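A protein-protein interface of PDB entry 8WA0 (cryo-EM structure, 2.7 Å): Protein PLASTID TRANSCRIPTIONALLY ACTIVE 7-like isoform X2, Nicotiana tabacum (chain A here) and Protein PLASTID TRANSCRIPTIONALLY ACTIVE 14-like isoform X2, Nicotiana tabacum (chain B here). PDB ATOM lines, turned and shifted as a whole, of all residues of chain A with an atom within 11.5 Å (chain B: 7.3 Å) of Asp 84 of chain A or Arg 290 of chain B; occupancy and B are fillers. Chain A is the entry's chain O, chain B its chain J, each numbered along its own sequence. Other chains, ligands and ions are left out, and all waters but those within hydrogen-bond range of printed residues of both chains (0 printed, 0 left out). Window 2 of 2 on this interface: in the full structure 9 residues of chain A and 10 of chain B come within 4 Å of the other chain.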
ATOM      1  N   ILE A  76     -22.401  28.742  -2.967  1.00  0.00           N
ATOM      2  CA  ILE A  76     -21.533  28.063  -2.035  1.00  0.00           C
ATOM      3  C   ILE A  76     -21.690  28.720  -0.685  1.00  0.00           C
ATOM      4  O   ILE A  76     -21.825  28.040   0.315  1.00  0.00           O
ATOM      5  CB  ILE A  76     -20.091  28.053  -2.529  1.00  0.00           C
ATOM      6  CG1 ILE A  76     -20.000  27.273  -3.835  1.00  0.00           C
ATOM      7  CG2 ILE A  76     -19.167  27.436  -1.497  1.00  0.00           C
ATOM      8  CD1 ILE A  76     -18.626  27.290  -4.456  1.00  0.00           C
ATOM      9  N   HIS A  77     -21.703  30.035  -0.637  1.00  0.00           N
ATOM     10  CA  HIS A  77     -21.939  30.760   0.589  1.00  0.00           C
ATOM     11  C   HIS A  77     -23.220  30.514   1.338  1.00  0.00           C
ATOM     12  O   HIS A  77     -23.171  30.438   2.526  1.00  0.00           O
ATOM     13  CB  HIS A  77     -21.840  32.213   0.320  1.00  0.00           C
ATOM     14  CG  HIS A  77     -20.440  32.725   0.213  1.00  0.00           C
ATOM     15  ND1 HIS A  77     -19.788  33.321   1.269  1.00  0.00           N
ATOM     16  CD2 HIS A  77     -19.578  32.764  -0.829  1.00  0.00           C
ATOM     17  CE1 HIS A  77     -18.582  33.698   0.884  1.00  0.00           C
ATOM     18  NE2 HIS A  77     -18.429  33.368  -0.383  1.00  0.00           N
ATOM     19  N   ARG A  78     -24.347  30.352   0.679  1.00  0.00           N
ATOM     20  CA  ARG A  78     -25.600  30.047   1.313  1.00  0.00           C
ATOM     21  C   ARG A  78     -25.456  28.773   1.998  1.00  0.00           C
ATOM     22  O   ARG A  78     -26.007  28.565   3.058  1.00  0.00           O
ATOM     23  CB  ARG A  78     -26.730  30.025   0.331  1.00  0.00           C
ATOM     24  N   LEU A  79     -24.882  27.818   1.331  1.00  0.00           N
ATOM     25  CA  LEU A  79     -24.814  26.489   1.835  1.00  0.00           C
ATOM     26  C   LEU A  79     -23.901  26.281   2.972  1.00  0.00           C
ATOM     27  O   LEU A  79     -24.085  25.355   3.725  1.00  0.00           O
ATOM     28  CB  LEU A  79     -24.521  25.573   0.672  1.00  0.00           C
ATOM     29  CG  LEU A  79     -25.538  25.367  -0.425  1.00  0.00           C
ATOM     30  CD1 LEU A  79     -24.958  24.430  -1.458  1.00  0.00           C
ATOM     31  CD2 LEU A  79     -26.829  24.814   0.135  1.00  0.00           C
ATOM     32  N   LEU A  80     -22.938  27.146   3.142  1.00  0.00           N
ATOM     33  CA  LEU A  80     -22.012  27.054   4.228  1.00  0.00           C
ATOM     34  C   LEU A  80     -22.524  27.788   5.436  1.00  0.00           C
ATOM     35  O   LEU A  80     -21.850  27.826   6.452  1.00  0.00           O
ATOM     36  CB  LEU A  80     -20.617  27.490   3.799  1.00  0.00           C
ATOM     37  CG  LEU A  80     -19.718  26.462   3.144  1.00  0.00           C
ATOM     38  CD1 LEU A  80     -18.499  27.152   2.569  1.00  0.00           C
ATOM     39  CD2 LEU A  80     -19.315  25.411   4.159  1.00  0.00           C
ATOM     40  N   LEU A  81     -23.704  28.360   5.359  1.00  0.00           N
ATOM     41  CA  LEU A  81     -24.303  29.089   6.442  1.00  0.00           C
ATOM     42  C   LEU A  81     -25.133  28.166   7.213  1.00  0.00           C
ATOM     43  O   LEU A  81     -25.813  28.567   8.114  1.00  0.00           O
ATOM     44  CB  LEU A  81     -25.159  30.245   5.949  1.00  0.00           C
ATOM     45  CG  LEU A  81     -24.455  31.443   5.347  1.00  0.00           C
ATOM     46  CD1 LEU A  81     -25.446  32.344   4.639  1.00  0.00           C
ATOM     47  CD2 LEU A  81     -23.649  32.195   6.389  1.00  0.00           C
ATOM     48  N   ASN A  82     -25.115  26.914   6.848  1.00  0.00           N
ATOM     49  CA  ASN A  82     -25.837  25.926   7.567  1.00  0.00           C
ATOM     50  C   ASN A  82     -24.892  24.991   8.247  1.00  0.00           C
ATOM     51  O   ASN A  82     -25.332  24.081   8.896  1.00  0.00           O
ATOM     52  CB  ASN A  82     -26.673  25.150   6.588  1.00  0.00           C
ATOM     53  CG  ASN A  82     -27.711  25.988   5.897  1.00  0.00           C
ATOM     54  OD1 ASN A  82     -28.068  25.713   4.756  1.00  0.00           O
ATOM     55  ND2 ASN A  82     -28.211  27.012   6.580  1.00  0.00           N
ATOM     56  N   GLU A  83     -23.590  25.224   8.169  1.00  0.00           N
ATOM     57  CA  GLU A  83     -22.602  24.282   8.675  1.00  0.00           C
ATOM     58  C   GLU A  83     -21.546  24.750   9.613  1.00  0.00           C
ATOM     59  O   GLU A  83     -20.868  25.708   9.312  1.00  0.00           O
ATOM     60  CB  GLU A  83     -21.851  23.791   7.463  1.00  0.00           C
ATOM     61  CG  GLU A  83     -22.094  22.344   7.097  1.00  0.00           C
ATOM     62  CD  GLU A  83     -23.316  22.156   6.226  1.00  0.00           C
ATOM     63  OE1 GLU A  83     -23.836  21.023   6.166  1.00  0.00           O
ATOM     64  OE2 GLU A  83     -23.758  23.139   5.599  1.00  0.00           O
ATOM     65  N   ASP A  84     -21.361  24.090  10.744  1.00  0.00           N
ATOM     66  CA  ASP A  84     -20.243  24.417  11.629  1.00  0.00           C
ATOM     67  C   ASP A  84     -18.852  24.079  11.150  1.00  0.00           C
ATOM     68  O   ASP A  84     -17.974  24.905  11.257  1.00  0.00           O
ATOM     69  CB  ASP A  84     -20.429  23.861  13.002  1.00  0.00           C
ATOM     70  CG  ASP A  84     -19.616  24.597  14.042  1.00  0.00           C
ATOM     71  OD1 ASP A  84     -19.332  25.795  13.843  1.00  0.00           O
ATOM     72  OD2 ASP A  84     -19.266  23.980  15.069  1.00  0.00           O
ATOM     73  N   ASN A  85     -18.625  22.918  10.573  1.00  0.00           N
ATOM     74  CA  ASN A  85     -17.316  22.658  10.047  1.00  0.00           C
ATOM     75  C   ASN A  85     -17.308  22.644   8.555  1.00  0.00           C
ATOM     76  O   ASN A  85     -18.050  21.904   7.952  1.00  0.00           O
ATOM     77  CB  ASN A  85     -16.690  21.421  10.653  1.00  0.00           C
ATOM     78  CG  ASN A  85     -15.195  21.490  10.716  1.00  0.00           C
ATOM     79  OD1 ASN A  85     -14.567  22.307  10.053  1.00  0.00           O
ATOM     80  ND2 ASN A  85     -14.613  20.631  11.521  1.00  0.00           N
ATOM     81  N   ARG A  86     -16.517  23.483   7.941  1.00  0.00           N
ATOM     82  CA  ARG A  86     -16.377  23.491   6.532  1.00  0.00           C
ATOM     83  C   ARG A  86     -15.765  22.277   6.035  1.00  0.00           C
ATOM     84  O   ARG A  86     -16.118  21.798   4.979  1.00  0.00           O
ATOM     85  CB  ARG A  86     -15.630  24.692   6.059  1.00  0.00           C
ATOM     86  CG  ARG A  86     -14.425  25.106   6.863  1.00  0.00           C
ATOM     87  CD  ARG A  86     -13.971  26.474   6.394  1.00  0.00           C
ATOM     88  NE  ARG A  86     -12.585  26.737   6.743  1.00  0.00           N
ATOM     89  CZ  ARG A  86     -12.196  27.375   7.838  1.00  0.00           C
ATOM     90  NH1 ARG A  86     -13.096  27.829   8.699  1.00  0.00           N
ATOM     91  NH2 ARG A  86     -10.906  27.567   8.072  1.00  0.00           N
ATOM     92  N   PHE A  87     -14.843  21.743   6.769  1.00  0.00           N
ATOM     93  CA  PHE A  87     -14.104  20.596   6.330  1.00  0.00           C
ATOM     94  C   PHE A  87     -14.970  19.392   6.130  1.00  0.00           C
ATOM     95  O   PHE A  87     -14.754  18.655   5.193  1.00  0.00           O
ATOM     96  CB  PHE A  87     -12.932  20.372   7.227  1.00  0.00           C
ATOM     97  CG  PHE A  87     -12.030  21.548   7.384  1.00  0.00           C
ATOM     98  CD1 PHE A  87     -11.422  22.121   6.303  1.00  0.00           C
ATOM     99  CD2 PHE A  87     -11.732  22.024   8.631  1.00  0.00           C
ATOM    100  CE1 PHE A  87     -10.568  23.184   6.460  1.00  0.00           C
ATOM    101  CE2 PHE A  87     -10.886  23.088   8.800  1.00  0.00           C
ATOM    102  CZ  PHE A  87     -10.299  23.665   7.713  1.00  0.00           C
ATOM    103  N   ASP A  88     -15.956  19.172   6.958  1.00  0.00           N
ATOM    104  CA  ASP A  88     -16.901  18.122   6.785  1.00  0.00           C
ATOM    105  C   ASP A  88     -17.790  18.254   5.597  1.00  0.00           C
ATOM    106  O   ASP A  88     -18.094  17.269   4.972  1.00  0.00           O
ATOM    107  CB  ASP A  88     -17.712  18.015   8.028  1.00  0.00           C
ATOM    108  CG  ASP A  88     -16.894  17.622   9.223  1.00  0.00           C
ATOM    109  OD1 ASP A  88     -15.715  17.251   9.048  1.00  0.00           O
ATOM    110  OD2 ASP A  88     -17.429  17.676  10.347  1.00  0.00           O
ATOM    111  N   PHE A  89     -18.233  19.443   5.269  1.00  0.00           N
ATOM    112  CA  PHE A  89     -19.040  19.680   4.112  1.00  0.00           C
ATOM    113  C   PHE A  89     -18.300  19.381   2.844  1.00  0.00           C
ATOM    114  O   PHE A  89     -18.883  18.830   1.932  1.00  0.00           O
ATOM    115  CB  PHE A  89     -19.577  21.076   4.209  1.00  0.00           C
ATOM    116  CG  PHE A  89     -20.588  21.457   3.186  1.00  0.00           C
ATOM    117  CD1 PHE A  89     -21.858  20.942   3.222  1.00  0.00           C
ATOM    118  CD2 PHE A  89     -20.287  22.412   2.240  1.00  0.00           C
ATOM    119  CE1 PHE A  89     -22.797  21.328   2.298  1.00  0.00           C
ATOM    120  CE2 PHE A  89     -21.217  22.804   1.315  1.00  0.00           C
ATOM    121  CZ  PHE A  89     -22.474  22.259   1.344  1.00  0.00           C
ATOM    122  N   VAL A  90     -17.032  19.682   2.757  1.00  0.00           N
ATOM    123  CA  VAL A  90     -16.243  19.334   1.606  1.00  0.00           C
ATOM    124  C   VAL A  90     -16.216  17.837   1.452  1.00  0.00           C
ATOM    125  O   VAL A  90     -16.411  17.331   0.361  1.00  0.00           O
ATOM    126  CB  VAL A  90     -14.840  19.942   1.691  1.00  0.00           C
ATOM    127  CG1 VAL A  90     -13.909  19.349   0.660  1.00  0.00           C
ATOM    128  CG2 VAL A  90     -14.897  21.446   1.575  1.00  0.00           C
ATOM    129  N   ASN A  91     -16.045  17.106   2.528  1.00  0.00           N
ATOM    130  CA  ASN A  91     -16.092  15.666   2.499  1.00  0.00           C
ATOM    131  C   ASN A  91     -17.439  15.087   2.135  1.00  0.00           C
ATOM    132  O   ASN A  91     -17.483  14.115   1.415  1.00  0.00           O
ATOM    133  CB  ASN A  91     -15.531  15.083   3.774  1.00  0.00           C
ATOM    134  CG  ASN A  91     -14.071  15.382   3.962  1.00  0.00           C
ATOM    135  OD1 ASN A  91     -13.365  15.700   3.014  1.00  0.00           O
ATOM    136  ND2 ASN A  91     -13.608  15.276   5.187  1.00  0.00           N
ATOM    137  N   GLU A  92     -18.546  15.635   2.586  1.00  0.00           N
ATOM    138  CA  GLU A  92     -19.845  15.173   2.143  1.00  0.00           C
ATOM    139  C   GLU A  92     -20.119  15.343   0.673  1.00  0.00           C
ATOM    140  O   GLU A  92     -20.609  14.423   0.042  1.00  0.00           O
ATOM    141  CB  GLU A  92     -20.908  15.896   2.897  1.00  0.00           C
ATOM    142  CG  GLU A  92     -22.330  15.530   2.542  1.00  0.00           C
ATOM    143  CD  GLU A  92     -23.331  16.386   3.285  1.00  0.00           C
ATOM    144  OE1 GLU A  92     -22.904  17.159   4.165  1.00  0.00           O
ATOM    145  OE2 GLU A  92     -24.541  16.287   2.988  1.00  0.00           O
ATOM    146  N   LEU B 147     -32.857  37.993  14.474  1.00  0.00           N
ATOM    147  CA  LEU B 147     -32.842  38.125  15.928  1.00  0.00           C
ATOM    148  C   LEU B 147     -33.340  39.447  16.446  1.00  0.00           C
ATOM    149  O   LEU B 147     -34.014  39.499  17.460  1.00  0.00           O
ATOM    150  CB  LEU B 147     -31.454  37.861  16.484  1.00  0.00           C
ATOM    151  CG  LEU B 147     -31.195  37.935  17.988  1.00  0.00           C
ATOM    152  CD1 LEU B 147     -32.018  36.907  18.743  1.00  0.00           C
ATOM    153  CD2 LEU B 147     -29.718  37.739  18.270  1.00  0.00           C
ATOM    154  N   GLN B 288     -32.968  26.392  22.232  1.00  0.00           N
ATOM    155  CA  GLN B 288     -31.591  26.602  22.644  1.00  0.00           C
ATOM    156  C   GLN B 288     -30.919  27.419  21.591  1.00  0.00           C
ATOM    157  O   GLN B 288     -30.990  27.083  20.423  1.00  0.00           O
ATOM    158  CB  GLN B 288     -30.861  25.281  22.765  1.00  0.00           C
ATOM    159  CG  GLN B 288     -29.494  25.402  23.403  1.00  0.00           C
ATOM    160  CD  GLN B 288     -28.715  24.113  23.354  1.00  0.00           C
ATOM    161  OE1 GLN B 288     -27.877  23.850  24.212  1.00  0.00           O
ATOM    162  NE2 GLN B 288     -28.994  23.294  22.351  1.00  0.00           N
ATOM    163  N   MET B 289     -30.260  28.493  21.980  1.00  0.00           N
ATOM    164  CA  MET B 289     -29.682  29.368  20.989  1.00  0.00           C
ATOM    165  C   MET B 289     -28.212  29.626  21.163  1.00  0.00           C
ATOM    166  O   MET B 289     -27.731  29.735  22.272  1.00  0.00           O
ATOM    167  CB  MET B 289     -30.435  30.683  20.963  1.00  0.00           C
ATOM    168  CG  MET B 289     -30.691  31.310  22.312  1.00  0.00           C
ATOM    169  SD  MET B 289     -31.385  32.946  22.063  1.00  0.00           S
ATOM    170  CE  MET B 289     -32.728  32.547  20.958  1.00  0.00           C
ATOM    171  N   ARG B 290     -27.488  29.709  20.064  1.00  0.00           N
ATOM    172  CA  ARG B 290     -26.081  30.005  20.131  1.00  0.00           C
ATOM    173  C   ARG B 290     -25.861  31.332  19.485  1.00  0.00           C
ATOM    174  O   ARG B 290     -26.077  31.476  18.294  1.00  0.00           O
ATOM    175  CB  ARG B 290     -25.278  28.962  19.386  1.00  0.00           C
ATOM    176  CG  ARG B 290     -23.792  29.251  19.328  1.00  0.00           C
ATOM    177  CD  ARG B 290     -23.070  28.199  18.514  1.00  0.00           C
ATOM    178  NE  ARG B 290     -21.750  28.655  18.102  1.00  0.00           N
ATOM    179  CZ  ARG B 290     -20.903  27.925  17.390  1.00  0.00           C
ATOM    180  NH1 ARG B 290     -21.237  26.701  17.015  1.00  0.00           N
ATOM    181  NH2 ARG B 290     -19.722  28.419  17.053  1.00  0.00           N
ATOM    182  N   ILE B 291     -25.449  32.318  20.262  1.00  0.00           N
ATOM    183  CA  ILE B 291     -25.142  33.603  19.699  1.00  0.00           C
ATOM    184  C   ILE B 291     -23.673  33.699  19.990  1.00  0.00           C
ATOM    185  O   ILE B 291     -23.257  33.558  21.130  1.00  0.00           O
ATOM    186  CB  ILE B 291     -25.972  34.717  20.331  1.00  0.00           C
ATOM    187  N   GLY B 292     -22.863  33.916  18.970  1.00  0.00           N
ATOM    188  CA  GLY B 292     -21.432  33.884  19.176  1.00  0.00           C
ATOM    189  C   GLY B 292     -20.986  32.516  19.635  1.00  0.00           C
ATOM    190  O   GLY B 292     -21.261  31.529  18.973  1.00  0.00           O
ATOM    191  N   ALA B 293     -20.254  32.445  20.732  1.00  0.00           N
ATOM    192  CA  ALA B 293     -19.818  31.176  21.264  1.00  0.00           C
ATOM    193  C   ALA B 293     -20.630  30.717  22.450  1.00  0.00           C
ATOM    194  O   ALA B 293     -20.318  29.699  23.045  1.00  0.00           O
ATOM    195  CB  ALA B 293     -18.381  31.290  21.667  1.00  0.00           C
ATOM    196  N   LEU B 294     -21.663  31.454  22.816  1.00  0.00           N
ATOM    197  CA  LEU B 294     -22.424  31.111  24.002  1.00  0.00           C
ATOM    198  C   LEU B 294     -23.632  30.288  23.664  1.00  0.00           C
ATOM    199  O   LEU B 294     -24.485  30.752  22.931  1.00  0.00           O
ATOM    200  CB  LEU B 294     -22.875  32.385  24.700  1.00  0.00           C
ATOM    201  CG  LEU B 294     -23.690  32.247  25.979  1.00  0.00           C
ATOM    202  CD1 LEU B 294     -22.821  31.680  27.087  1.00  0.00           C
ATOM    203  CD2 LEU B 294     -24.250  33.599  26.378  1.00  0.00           C
ATOM    204  N   VAL B 295     -23.727  29.067  24.176  1.00  0.00           N
ATOM    205  CA  VAL B 295     -24.900  28.311  23.948  1.00  0.00           C
ATOM    206  C   VAL B 295     -25.727  28.373  25.176  1.00  0.00           C
ATOM    207  O   VAL B 295     -25.277  27.983  26.222  1.00  0.00           O
ATOM    208  CB  VAL B 295     -24.611  26.908  23.478  1.00  0.00           C
ATOM    209  CG1 VAL B 295     -25.803  26.357  22.725  1.00  0.00           C
ATOM    210  CG2 VAL B 295     -23.394  26.895  22.581  1.00  0.00           C
ATOM    211  N   GLN B 296     -26.940  28.886  25.061  1.00  0.00           N
ATOM    212  CA  GLN B 296     -27.811  29.032  26.202  1.00  0.00           C
ATOM    213  C   GLN B 296     -29.183  28.549  25.851  1.00  0.00           C
ATOM    214  O   GLN B 296     -29.492  28.389  24.686  1.00  0.00           O
ATOM    215  CB  GLN B 296     -27.904  30.493  26.592  1.00  0.00           C
ATOM    216  CG  GLN B 296     -28.622  31.375  25.595  1.00  0.00           C
ATOM    217  CD  GLN B 296     -28.912  32.743  26.158  1.00  0.00           C
ATOM    218  OE1 GLN B 296     -28.292  33.166  27.130  1.00  0.00           O
ATOM    219  NE2 GLN B 296     -29.859  33.444  25.552  1.00  0.00           N
ATOM    220  N   TRP B 320     -32.538  27.009  14.690  1.00  0.00           N
ATOM    221  CA  TRP B 320     -31.674  28.166  14.788  1.00  0.00           C
ATOM    222  C   TRP B 320     -30.468  28.134  13.872  1.00  0.00           C
ATOM    223  O   TRP B 320     -29.675  27.221  13.965  1.00  0.00           O
ATOM    224  CB  TRP B 320     -31.208  28.318  16.225  1.00  0.00           C
ATOM    225  CG  TRP B 320     -30.410  29.502  16.528  1.00  0.00           C
ATOM    226  CD1 TRP B 320     -29.065  29.572  16.608  1.00  0.00           C
ATOM    227  CD2 TRP B 320     -30.898  30.799  16.827  1.00  0.00           C
ATOM    228  NE1 TRP B 320     -28.677  30.838  16.917  1.00  0.00           N
ATOM    229  CE2 TRP B 320     -29.791  31.614  17.053  1.00  0.00           C
ATOM    230  CE3 TRP B 320     -32.170  31.358  16.909  1.00  0.00           C
ATOM    231  CZ2 TRP B 320     -29.909  32.948  17.360  1.00  0.00           C
ATOM    232  CZ3 TRP B 320     -32.286  32.673  17.207  1.00  0.00           C
ATOM    233  CH2 TRP B 320     -31.166  33.460  17.433  1.00  0.00           C
ATOM    234  N   ARG B 321     -30.298  29.105  12.993  1.00  0.00           N
ATOM    235  CA  ARG B 321     -29.119  29.203  12.157  1.00  0.00           C
ATOM    236  C   ARG B 321     -28.229  30.204  12.817  1.00  0.00           C
ATOM    237  O   ARG B 321     -28.542  31.372  12.850  1.00  0.00           O
ATOM    238  CB  ARG B 321     -29.451  29.645  10.739  1.00  0.00           C
ATOM    239  CG  ARG B 321     -28.224  29.927   9.913  1.00  0.00           C
ATOM    240  CD  ARG B 321     -28.597  30.821   8.767  1.00  0.00           C
ATOM    241  NE  ARG B 321     -29.668  30.220   8.005  1.00  0.00           N
ATOM    242  CZ  ARG B 321     -30.215  30.775   6.938  1.00  0.00           C
ATOM    243  NH1 ARG B 321     -29.797  31.947   6.509  1.00  0.00           N
ATOM    244  NH2 ARG B 321     -31.176  30.146   6.300  1.00  0.00           N
ATOM    245  N   PHE B 322     -27.119  29.778  13.347  1.00  0.00           N
ATOM    246  CA  PHE B 322     -26.246  30.640  14.089  1.00  0.00           C
ATOM    247  C   PHE B 322     -25.519  31.696  13.371  1.00  0.00           C
ATOM    248  O   PHE B 322     -25.374  32.788  13.885  1.00  0.00           O
ATOM    249  CB  PHE B 322     -25.358  29.852  15.079  1.00  0.00           C
ATOM    250  CG  PHE B 322     -24.176  29.160  14.488  1.00  0.00           C
ATOM    251  CD1 PHE B 322     -24.288  27.889  13.983  1.00  0.00           C
ATOM    252  CD2 PHE B 322     -22.935  29.747  14.522  1.00  0.00           C
ATOM    253  CE1 PHE B 322     -23.197  27.245  13.454  1.00  0.00           C
ATOM    254  CE2 PHE B 322     -21.838  29.108  14.001  1.00  0.00           C
ATOM    255  CZ  PHE B 322     -21.968  27.853  13.465  1.00  0.00           C
ATOM    256  N   LYS B 323     -25.049  31.429  12.205  1.00  0.00           N
ATOM    257  CA  LYS B 323     -24.221  32.351  11.540  1.00  0.00           C
ATOM    258  C   LYS B 323     -24.802  33.673  11.155  1.00  0.00           C
ATOM    259  O   LYS B 323     -24.119  34.671  11.248  1.00  0.00           O
ATOM    260  CB  LYS B 323     -23.617  31.635  10.379  1.00  0.00           C
ATOM    261  CG  LYS B 323     -22.579  30.586  10.711  1.00  0.00           C
ATOM    262  CD  LYS B 323     -21.743  30.276   9.486  1.00  0.00           C
ATOM    263  CE  LYS B 323     -20.735  29.179   9.738  1.00  0.00           C
ATOM    264  NZ  LYS B 323     -19.756  29.563  10.786  1.00  0.00           N
ATOM    265  N   ARG B 325     -27.558  34.694  12.539  1.00  0.00           N
ATOM    266  CA  ARG B 325     -28.408  34.987  13.669  1.00  0.00           C
ATOM    267  C   ARG B 325     -29.885  34.973  13.446  1.00  0.00           C
ATOM    268  O   ARG B 325     -30.562  35.864  13.889  1.00  0.00           O
ATOM    269  CB  ARG B 325     -27.839  36.114  14.486  1.00  0.00           C
ATOM    270  CG  ARG B 325     -26.332  36.040  14.580  1.00  0.00           C
ATOM    271  CD  ARG B 325     -25.842  36.150  15.998  1.00  0.00           C
ATOM    272  NE  ARG B 325     -25.814  37.525  16.446  1.00  0.00           N
ATOM    273  CZ  ARG B 325     -24.762  38.102  17.001  1.00  0.00           C
ATOM    274  NH1 ARG B 325     -23.650  37.422  17.177  1.00  0.00           N
ATOM    275  NH2 ARG B 325     -24.828  39.361  17.390  1.00  0.00           N
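NE of Arg 290 of chain B lies within hydrogen-bond range of O of Gly 292 of chain B (3.0 Å).
The backbone carbonyl oxygen (O) of Arg 290 of chain B lies within hydrogen-bond range of the indole nitrogen (NE1) of Trp 320 of chain B.
Of the 17 printed residues of chain A, 5 touch a printed residue of chain B.
Of the 15 printed residues of chain B, 4 touch a printed residue of chain A.
Printed residues of chain B that touch a printed residue of chain A: Arg 290, Arg 321, Phe 322 and Lys 323.
Hydrophobic or aromatic side chains of chain B that line the printed part of chain A: Phe 322.
Among the printed residues, 6 pairs touch across the chains.
Of chain B, only Arg 290 and Phe 322 come within 4 Å of Asp 84 of chain A.
Arg 290 of chain B touches just one residue of chain A: Asp 84 (3.8 Å).
No residue of chain A comes within 4 Å of Gln 288 of chain B.
No residue of chain A comes within 4 Å of Met 289 of chain B.
No residue of chain A comes within 4 Å of Ile 291 of chain B.
No residue of chain A comes within 4 Å of Gly 292 of chain B.
No residue of chain A comes within 4 Å of Val 295 of chain B.
Phe 322 of chain B touches one residue of chain A.
Of the printed residues of chain A, Arg 321 of chain B touches Leu 81 (3.3 Å) and Asn 82 (3.8 Å).
Of the printed residues of chain B, Leu 81 of chain A touches Arg 321 (3.3 Å).
Printed residues of chain B within 4 Å of Glu 83 of chain A: Lys 323 (3.5 Å).
Leu 294 of chain B touches none of the printed residues of chain A.
The nearest residue of chain A that does not touch Arg 290 of chain B is Glu 83 of chain A (7.7 Å).
Among the printed residues, merely in contact across the chains: Leu 80 of chain A with Lys 323 of chain B, Leu 81 of chain A with Arg 321 of chain B, Asn 82 of chain A with Arg 321 of chain B, Glu 83 of chain A with Lys 323 of chain B and Asp 84 of chain A with Phe 322 of chain B.
NH1 of Arg 290 of chain B lies within salt-bridge range of OD1 of Asp 84 of chain A (3.8 Å).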
